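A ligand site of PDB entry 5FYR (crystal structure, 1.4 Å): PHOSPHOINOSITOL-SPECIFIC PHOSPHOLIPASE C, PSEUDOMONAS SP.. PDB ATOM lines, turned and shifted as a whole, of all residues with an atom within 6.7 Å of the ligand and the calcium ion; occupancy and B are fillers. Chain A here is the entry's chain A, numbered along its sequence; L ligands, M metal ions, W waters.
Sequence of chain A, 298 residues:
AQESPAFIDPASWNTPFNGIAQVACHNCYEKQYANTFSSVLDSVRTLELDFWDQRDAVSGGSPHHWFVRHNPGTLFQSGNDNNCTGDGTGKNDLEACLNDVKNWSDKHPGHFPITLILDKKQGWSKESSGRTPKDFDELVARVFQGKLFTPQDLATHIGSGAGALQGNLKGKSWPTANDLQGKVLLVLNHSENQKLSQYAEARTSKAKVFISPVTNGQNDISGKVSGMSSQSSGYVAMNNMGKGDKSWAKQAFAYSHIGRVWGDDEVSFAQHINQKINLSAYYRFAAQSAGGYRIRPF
ND2 of Asn 189 lies within hydrogen-bond range of O4 of the ligand.
An oxygen (O4) of the ligand lies within hydrogen-bond range of the guanidinium group (NH1) of Arg 260 (2.9 Å).
O4 of the ligand is in hydrogen-bond range of ND2 of Asn 240, 3.0 Å away.
An oxygen (O2) of the ligand sits close to a ring nitrogen (NE2) of His 26, 3.3 Å away.
The side-chain carboxylate (OD2) of Asp 50 sits close to the side-chain amino group (NZ) of Lys 121 (3.96 Å).
The side-chain hydroxyl (OH) of Tyr 29 sits close to the side-chain carboxylate (OD2) of Asp 50 (2.8 Å).
OD2 of Asp 119 sits close to NZ of Lys 121, 3.0 Å away.
The backbone carbonyl oxygen (O) of Leu 49 lies within hydrogen-bond range of the backbone NH (N) of Asp 119, 2.8 Å away.
The side-chain amide nitrogen (ND2) of Asn 189 lies close to the side-chain amide nitrogen (ND2) of Asn 240.
O of Asn 189 is in hydrogen-bond range of N of Lys 120 (2.8 Å).
The guanidinium group of Arg 260 sits at hydrogen-bond distance from the side-chain amide oxygen of Asn 240 (3.0 Å).
ND2 of Asn 240 sits close to NE1 of Trp 262 (3.5 Å).
NZ of Lys 121 touches O1 of the ligand, 3.9 Å away.
Trp 262 touches the ligand (CG to C3, 3.6 Å).
Hydrophobic or aromatic side chains that line the ligand: His 26 and Trp 262.
Within 4 Å of the ligand: His 26, Asn 27, Glu 48, Asp 119, Lys 121, Asn 189, Asn 240, Arg 260 and Trp 262.
Four residues have an atom within 4 Å of the calcium ion: Asn 27, Glu 48, Asp 50 and Asp 119.
The nearest printed residue that does not touch the calcium ion is Lys 121 (4.1 Å).
The calcium ion is bound by the side-chain carboxylate (OD1) of Asp 50 (2.3 Å), the side-chain carboxylate (OE2) of Glu 48 (2.3 Å), an oxygen (O2) of the ligand (2.4 Å), the side-chain amide oxygen (OD1) of Asn 27 (2.4 Å), the side-chain carboxylate (OD2) of Asp 119 (2.4 Å), water W4 (2.5 Å) and the side-chain carboxylate (OD2) of Asp 50 (2.7 Å).
Water W4 lies within hydrogen-bond range of the side-chain amino group of Lys 121 (2.9 Å) and an oxygen (O1) of the ligand (3.0 Å).
Water W2 lies within hydrogen-bond range of an oxygen (O1) of the ligand (2.7 Å) and a ring nitrogen (NE2) of His 26 (2.9 Å).
Water W3 lies within hydrogen-bond range of OD1 of Asp 119 (2.7 Å), O6 of the ligand (2.8 Å) and NZ of Lys 121 (2.9 Å).
Water W1 lies within hydrogen-bond range of an oxygen (O5) of the ligand, the side-chain amide nitrogen of Asn 240 and the backbone carbonyl oxygen of His 190.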
ATOM      1  N   CYS A  25     -25.570 -18.233  33.506  1.00  0.00           N
ATOM      2  CA  CYS A  25     -25.729 -19.365  34.381  1.00  0.00           C
ATOM      3  C   CYS A  25     -25.426 -20.690  33.690  1.00  0.00           C
ATOM      4  O   CYS A  25     -25.469 -20.793  32.431  1.00  0.00           O
ATOM      5  CB  CYS A  25     -27.131 -19.405  34.973  1.00  0.00           C
ATOM      6  SG  CYS A  25     -28.293 -20.390  34.050  1.00  0.00           S
ATOM      7  N   HIS A  26     -25.112 -21.704  34.491  1.00  0.00           N
ATOM      8  CA  HIS A  26     -25.075 -23.053  34.003  1.00  0.00           C
ATOM      9  C   HIS A  26     -26.109 -23.873  34.808  1.00  0.00           C
ATOM     10  O   HIS A  26     -25.985 -24.057  36.031  1.00  0.00           O
ATOM     11  CB  HIS A  26     -23.672 -23.632  34.199  1.00  0.00           C
ATOM     12  CG  HIS A  26     -23.492 -25.020  33.657  1.00  0.00           C
ATOM     13  ND1 HIS A  26     -22.277 -25.656  33.691  1.00  0.00           N
ATOM     14  CD2 HIS A  26     -24.336 -25.867  32.993  1.00  0.00           C
ATOM     15  CE1 HIS A  26     -22.386 -26.870  33.162  1.00  0.00           C
ATOM     16  NE2 HIS A  26     -23.623 -27.017  32.727  1.00  0.00           N
ATOM     17  N   ASN A  27     -27.156 -24.325  34.109  1.00  0.00           N
ATOM     18  CA  ASN A  27     -28.174 -25.170  34.708  1.00  0.00           C
ATOM     19  C   ASN A  27     -28.888 -24.506  35.864  1.00  0.00           C
ATOM     20  O   ASN A  27     -29.303 -25.153  36.824  1.00  0.00           O
ATOM     21  CB  ASN A  27     -27.652 -26.519  35.108  1.00  0.00           C
ATOM     22  CG  ASN A  27     -27.385 -27.467  33.963  1.00  0.00           C
ATOM     23  OD1 ASN A  27     -27.510 -27.165  32.786  1.00  0.00           O
ATOM     24  ND2 ASN A  27     -27.056 -28.659  34.330  1.00  0.00           N
ATOM     25  N   TYR A  29     -31.833 -23.548  36.410  1.00  0.00           N
ATOM     26  CA  TYR A  29     -33.149 -24.100  36.716  1.00  0.00           C
ATOM     27  C   TYR A  29     -33.105 -25.103  37.865  1.00  0.00           C
ATOM     28  O   TYR A  29     -34.165 -25.462  38.412  1.00  0.00           O
ATOM     29  CB  TYR A  29     -33.749 -24.825  35.483  1.00  0.00           C
ATOM     30  CG  TYR A  29     -33.009 -26.055  35.093  1.00  0.00           C
ATOM     31  CD1 TYR A  29     -33.304 -27.278  35.713  1.00  0.00           C
ATOM     32  CD2 TYR A  29     -31.959 -26.017  34.182  1.00  0.00           C
ATOM     33  CE1 TYR A  29     -32.583 -28.398  35.394  1.00  0.00           C
ATOM     34  CE2 TYR A  29     -31.206 -27.129  33.891  1.00  0.00           C
ATOM     35  CZ  TYR A  29     -31.513 -28.332  34.504  1.00  0.00           C
ATOM     36  OH  TYR A  29     -30.809 -29.495  34.264  1.00  0.00           O
ATOM     37  N   GLU A  48     -30.382 -20.779  31.418  1.00  0.00           N
ATOM     38  CA  GLU A  48     -30.391 -22.091  30.815  1.00  0.00           C
ATOM     39  C   GLU A  48     -31.540 -22.963  31.332  1.00  0.00           C
ATOM     40  O   GLU A  48     -31.808 -22.971  32.523  1.00  0.00           O
ATOM     41  CB  GLU A  48     -29.027 -22.774  31.063  1.00  0.00           C
ATOM     42  CG  GLU A  48     -28.892 -24.154  30.393  1.00  0.00           C
ATOM     43  CD  GLU A  48     -27.497 -24.769  30.533  1.00  0.00           C
ATOM     44  OE1 GLU A  48     -26.646 -24.242  31.296  1.00  0.00           O
ATOM     45  OE2 GLU A  48     -27.260 -25.844  29.887  1.00  0.00           O
ATOM     46  N   LEU A  49     -32.136 -23.734  30.428  1.00  0.00           N
ATOM     47  CA  LEU A  49     -33.152 -24.721  30.723  1.00  0.00           C
ATOM     48  C   LEU A  49     -32.791 -25.995  29.995  1.00  0.00           C
ATOM     49  O   LEU A  49     -32.593 -25.980  28.772  1.00  0.00           O
ATOM     50  CB  LEU A  49     -34.521 -24.227  30.250  1.00  0.00           C
ATOM     51  CG  LEU A  49     -35.095 -23.100  31.053  1.00  0.00           C
ATOM     52  CD1 LEU A  49     -36.197 -22.361  30.315  1.00  0.00           C
ATOM     53  CD2 LEU A  49     -35.573 -23.526  32.443  1.00  0.00           C
ATOM     54  N   ASP A  50     -32.793 -27.116  30.706  1.00  0.00           N
ATOM     55  CA  ASP A  50     -32.654 -28.443  30.088  1.00  0.00           C
ATOM     56  C   ASP A  50     -34.046 -29.036  29.926  1.00  0.00           C
ATOM     57  O   ASP A  50     -34.743 -29.198  30.907  1.00  0.00           O
ATOM     58  CB  ASP A  50     -31.794 -29.347  30.989  1.00  0.00           C
ATOM     59  CG  ASP A  50     -30.330 -28.894  31.081  1.00  0.00           C
ATOM     60  OD1 ASP A  50     -29.960 -27.877  30.477  1.00  0.00           O
ATOM     61  OD2 ASP A  50     -29.529 -29.474  31.786  1.00  0.00           O
ATOM     62  N   HIS A  70     -32.769 -32.156  35.211  1.00  0.00           N
ATOM     63  CA  HIS A  70     -31.407 -32.484  34.842  1.00  0.00           C
ATOM     64  C   HIS A  70     -31.185 -33.937  34.363  1.00  0.00           C
ATOM     65  O   HIS A  70     -30.645 -34.150  33.305  1.00  0.00           O
ATOM     66  CB  HIS A  70     -30.528 -32.191  36.069  1.00  0.00           C
ATOM     67  CG  HIS A  70     -29.079 -32.312  35.774  1.00  0.00           C
ATOM     68  ND1 HIS A  70     -28.208 -33.007  36.586  1.00  0.00           N
ATOM     69  CD2 HIS A  70     -28.361 -31.883  34.725  1.00  0.00           C
ATOM     70  CE1 HIS A  70     -26.999 -32.966  36.058  1.00  0.00           C
ATOM     71  NE2 HIS A  70     -27.067 -32.270  34.946  1.00  0.00           N
ATOM     72  N   ILE A 117     -30.696 -20.226  26.960  1.00  0.00           N
ATOM     73  CA  ILE A 117     -30.105 -21.405  26.370  1.00  0.00           C
ATOM     74  C   ILE A 117     -31.068 -22.554  26.659  1.00  0.00           C
ATOM     75  O   ILE A 117     -31.288 -22.928  27.823  1.00  0.00           O
ATOM     76  CB  ILE A 117     -28.733 -21.713  26.995  1.00  0.00           C
ATOM     77  CG1 ILE A 117     -27.750 -20.459  26.882  1.00  0.00           C
ATOM     78  CG2 ILE A 117     -28.213 -23.058  26.496  1.00  0.00           C
ATOM     79  CD1 ILE A 117     -27.552 -19.871  25.561  1.00  0.00           C
ATOM     80  N   ASP A 119     -31.430 -26.270  26.286  1.00  0.00           N
ATOM     81  CA  ASP A 119     -30.544 -27.387  26.130  1.00  0.00           C
ATOM     82  C   ASP A 119     -31.403 -28.658  25.985  1.00  0.00           C
ATOM     83  O   ASP A 119     -31.962 -29.143  26.978  1.00  0.00           O
ATOM     84  CB  ASP A 119     -29.595 -27.410  27.317  1.00  0.00           C
ATOM     85  CG  ASP A 119     -28.571 -28.512  27.239  1.00  0.00           C
ATOM     86  OD1 ASP A 119     -28.268 -28.970  26.130  1.00  0.00           O
ATOM     87  OD2 ASP A 119     -28.009 -28.897  28.312  1.00  0.00           O
ATOM     88  N   LYS A 120     -31.622 -29.077  24.742  1.00  0.00           N
ATOM     89  CA  LYS A 120     -32.526 -30.168  24.426  1.00  0.00           C
ATOM     90  C   LYS A 120     -31.863 -31.479  24.787  1.00  0.00           C
ATOM     91  O   LYS A 120     -30.701 -31.691  24.397  1.00  0.00           O
ATOM     92  CB  LYS A 120     -32.911 -30.111  22.957  1.00  0.00           C
ATOM     93  CG  LYS A 120     -34.101 -31.002  22.633  1.00  0.00           C
ATOM     94  CD  LYS A 120     -34.478 -30.908  21.138  1.00  0.00           C
ATOM     95  CE  LYS A 120     -35.904 -31.410  20.847  1.00  0.00           C
ATOM     96  NZ  LYS A 120     -36.337 -32.542  21.652  1.00  0.00           N
ATOM     97  N   LYS A 121     -32.590 -32.386  25.466  1.00  0.00           N
ATOM     98  CA  LYS A 121     -31.998 -33.611  25.963  1.00  0.00           C
ATOM     99  C   LYS A 121     -32.426 -34.894  25.245  1.00  0.00           C
ATOM    100  O   LYS A 121     -31.779 -35.933  25.410  1.00  0.00           O
ATOM    101  CB  LYS A 121     -32.280 -33.743  27.462  1.00  0.00           C
ATOM    102  CG  LYS A 121     -31.634 -32.639  28.293  1.00  0.00           C
ATOM    103  CD  LYS A 121     -30.100 -32.778  28.298  1.00  0.00           C
ATOM    104  CE  LYS A 121     -29.411 -31.726  29.129  1.00  0.00           C
ATOM    105  NZ  LYS A 121     -27.911 -31.841  29.054  1.00  0.00           N
ATOM    106  N   ASN A 189     -29.431 -25.798  22.068  1.00  0.00           N
ATOM    107  CA  ASN A 189     -28.264 -26.653  22.186  1.00  0.00           C
ATOM    108  C   ASN A 189     -28.734 -28.127  22.257  1.00  0.00           C
ATOM    109  O   ASN A 189     -29.890 -28.417  22.585  1.00  0.00           O
ATOM    110  CB  ASN A 189     -27.426 -26.440  23.465  1.00  0.00           C
ATOM    111  CG  ASN A 189     -26.750 -25.093  23.586  1.00  0.00           C
ATOM    112  OD1 ASN A 189     -26.635 -24.279  22.619  1.00  0.00           O
ATOM    113  ND2 ASN A 189     -26.321 -24.797  24.757  1.00  0.00           N
ATOM    114  N   HIS A 190     -27.848 -29.039  21.925  1.00  0.00           N
ATOM    115  CA  HIS A 190     -28.025 -30.492  22.082  1.00  0.00           C
ATOM    116  C   HIS A 190     -26.599 -31.063  22.033  1.00  0.00           C
ATOM    117  O   HIS A 190     -25.731 -30.492  21.386  1.00  0.00           O
ATOM    118  CB  HIS A 190     -28.911 -31.036  20.948  1.00  0.00           C
ATOM    119  CG  HIS A 190     -29.436 -32.404  21.195  1.00  0.00           C
ATOM    120  ND1 HIS A 190     -28.667 -33.525  21.009  1.00  0.00           N
ATOM    121  CD2 HIS A 190     -30.652 -32.872  21.588  1.00  0.00           C
ATOM    122  CE1 HIS A 190     -29.342 -34.608  21.313  1.00  0.00           C
ATOM    123  NE2 HIS A 190     -30.558 -34.251  21.653  1.00  0.00           N
ATOM    124  N   SER A 191     -26.399 -32.245  22.595  1.00  0.00           N
ATOM    125  CA  SER A 191     -25.108 -32.922  22.494  1.00  0.00           C
ATOM    126  C   SER A 191     -24.807 -33.376  21.082  1.00  0.00           C
ATOM    127  O   SER A 191     -23.672 -33.490  20.708  1.00  0.00           O
ATOM    128  CB  SER A 191     -25.038 -34.057  23.526  1.00  0.00           C
ATOM    129  OG  SER A 191     -25.864 -35.091  23.137  1.00  0.00           O
ATOM    130  N   VAL A 214     -22.321 -27.625  18.836  1.00  0.00           N
ATOM    131  CA  VAL A 214     -21.087 -28.053  19.472  1.00  0.00           C
ATOM    132  C   VAL A 214     -19.970 -27.718  18.498  1.00  0.00           C
ATOM    133  O   VAL A 214     -20.038 -28.092  17.317  1.00  0.00           O
ATOM    134  CB  VAL A 214     -21.085 -29.564  19.743  1.00  0.00           C
ATOM    135  CG1 VAL A 214     -19.735 -30.031  20.282  1.00  0.00           C
ATOM    136  CG2 VAL A 214     -22.189 -29.914  20.736  1.00  0.00           C
ATOM    137  N   ASN A 240     -21.318 -23.086  20.518  1.00  0.00           N
ATOM    138  CA  ASN A 240     -21.302 -23.583  21.911  1.00  0.00           C
ATOM    139  C   ASN A 240     -20.041 -24.445  22.127  1.00  0.00           C
ATOM    140  O   ASN A 240     -19.814 -25.387  21.392  1.00  0.00           O
ATOM    141  CB  ASN A 240     -22.565 -24.395  22.233  1.00  0.00           C
ATOM    142  CG  ASN A 240     -22.933 -24.366  23.736  1.00  0.00           C
ATOM    143  OD1 ASN A 240     -23.001 -23.302  24.387  1.00  0.00           O
ATOM    144  ND2 ASN A 240     -23.175 -25.537  24.282  1.00  0.00           N
ATOM    145  N   ARG A 260     -20.423 -19.196  23.392  1.00  0.00           N
ATOM    146  CA  ARG A 260     -20.658 -19.565  24.776  1.00  0.00           C
ATOM    147  C   ARG A 260     -19.704 -20.685  25.180  1.00  0.00           C
ATOM    148  O   ARG A 260     -19.503 -21.640  24.441  1.00  0.00           O
ATOM    149  CB  ARG A 260     -22.115 -20.047  24.964  1.00  0.00           C
ATOM    150  CG  ARG A 260     -22.467 -20.474  26.384  1.00  0.00           C
ATOM    151  CD  ARG A 260     -23.978 -20.585  26.577  1.00  0.00           C
ATOM    152  NE  ARG A 260     -24.409 -21.143  27.857  1.00  0.00           N
ATOM    153  CZ  ARG A 260     -24.381 -22.436  28.118  1.00  0.00           C
ATOM    154  NH1 ARG A 260     -23.932 -23.313  27.234  1.00  0.00           N
ATOM    155  NH2 ARG A 260     -24.873 -22.868  29.266  1.00  0.00           N
ATOM    156  N   TRP A 262     -19.010 -23.346  28.452  1.00  0.00           N
ATOM    157  CA  TRP A 262     -19.527 -23.947  29.670  1.00  0.00           C
ATOM    158  C   TRP A 262     -18.499 -24.918  30.232  1.00  0.00           C
ATOM    159  O   TRP A 262     -17.635 -25.400  29.511  1.00  0.00           O
ATOM    160  CB  TRP A 262     -20.852 -24.699  29.393  1.00  0.00           C
ATOM    161  CG  TRP A 262     -20.740 -25.781  28.351  1.00  0.00           C
ATOM    162  CD1 TRP A 262     -20.896 -25.632  27.005  1.00  0.00           C
ATOM    163  CD2 TRP A 262     -20.504 -27.165  28.566  1.00  0.00           C
ATOM    164  NE1 TRP A 262     -20.740 -26.820  26.368  1.00  0.00           N
ATOM    165  CE2 TRP A 262     -20.521 -27.789  27.288  1.00  0.00           C
ATOM    166  CE3 TRP A 262     -20.306 -27.962  29.694  1.00  0.00           C
ATOM    167  CZ2 TRP A 262     -20.291 -29.156  27.102  1.00  0.00           C
ATOM    168  CZ3 TRP A 262     -20.097 -29.330  29.500  1.00  0.00           C
ATOM    169  CH2 TRP A 262     -20.091 -29.900  28.222  1.00  0.00           C
ATOM    170  N   GLY A 263     -18.603 -25.152  31.541  1.00  0.00           N
ATOM    171  CA  GLY A 263     -17.745 -26.090  32.260  1.00  0.00           C
ATOM    172  C   GLY A 263     -16.397 -25.523  32.686  1.00  0.00           C
ATOM    173  O   GLY A 263     -15.548 -26.274  33.146  1.00  0.00           O
ATOM    174  N   ALA A 281     -20.541 -19.517  31.082  1.00  0.00           N
ATOM    175  CA  ALA A 281     -21.533 -20.172  31.913  1.00  0.00           C
ATOM    176  C   ALA A 281     -20.934 -20.689  33.201  1.00  0.00           C
ATOM    177  O   ALA A 281     -19.974 -21.463  33.161  1.00  0.00           O
ATOM    178  CB  ALA A 281     -22.214 -21.298  31.118  1.00  0.00           C
ATOM    179  N   TYR A 283     -21.919 -22.315  37.254  1.00  0.00           N
ATOM    180  CA  TYR A 283     -22.859 -22.771  38.249  1.00  0.00           C
ATOM    181  C   TYR A 283     -23.091 -21.714  39.297  1.00  0.00           C
ATOM    182  O   TYR A 283     -24.272 -21.380  39.638  1.00  0.00           O
ATOM    183  CB  TYR A 283     -22.366 -24.019  38.936  1.00  0.00           C
ATOM    184  CG  TYR A 283     -22.214 -25.240  38.059  1.00  0.00           C
ATOM    185  CD1 TYR A 283     -23.331 -25.847  37.493  1.00  0.00           C
ATOM    186  CD2 TYR A 283     -20.974 -25.802  37.800  1.00  0.00           C
ATOM    187  CE1 TYR A 283     -23.216 -26.969  36.712  1.00  0.00           C
ATOM    188  CE2 TYR A 283     -20.844 -26.918  37.003  1.00  0.00           C
ATOM    189  CZ  TYR A 283     -21.973 -27.539  36.484  1.00  0.00           C
ATOM    190  OH  TYR A 283     -21.845 -28.685  35.696  1.00  0.00           O
HETATM  191  C1  LIG L   1     -23.901 -29.476  28.758  1.00  0.00           C
HETATM  192  C2  LIG L   1     -24.073 -28.177  29.538  1.00  0.00           C
HETATM  193  C3  LIG L   1     -24.173 -26.948  28.707  1.00  0.00           C
HETATM  194  C4  LIG L   1     -24.917 -27.113  27.437  1.00  0.00           C
HETATM  195  C5  LIG L   1     -24.806 -28.387  26.707  1.00  0.00           C
HETATM  196  C6  LIG L   1     -24.718 -29.600  27.519  1.00  0.00           C
HETATM  197  O1  LIG L   1     -24.253 -30.505  29.689  1.00  0.00           O
HETATM  198  O2  LIG L   1     -25.309 -28.328  30.260  1.00  0.00           O
HETATM  199  O3  LIG L   1     -24.549 -25.802  29.470  1.00  0.00           O
HETATM  200  O4  LIG L   1     -24.886 -25.942  26.667  1.00  0.00           O
HETATM  201  O5  LIG L   1     -25.545 -28.496  25.502  1.00  0.00           O
HETATM  202  O6  LIG L   1     -24.553 -30.786  26.816  1.00  0.00           O
HETATM  203 CA    CA M   1     -27.669 -28.014  30.541  1.00  0.00          CA
HETATM  204  O   HOH W   1     -23.958 -28.108  23.171  1.00  0.00           O
HETATM  205  O   HOH W   2     -24.433 -29.741  32.256  1.00  0.00           O
HETATM  206  O   HOH W   3     -27.219 -31.452  26.316  1.00  0.00           O
HETATM  207  O   HOH W   4     -26.807 -30.247  31.198  1.00  0.00           O
HETATM  208  O   HOH W   5     -23.225 -30.468  24.246  1.00  0.00           O
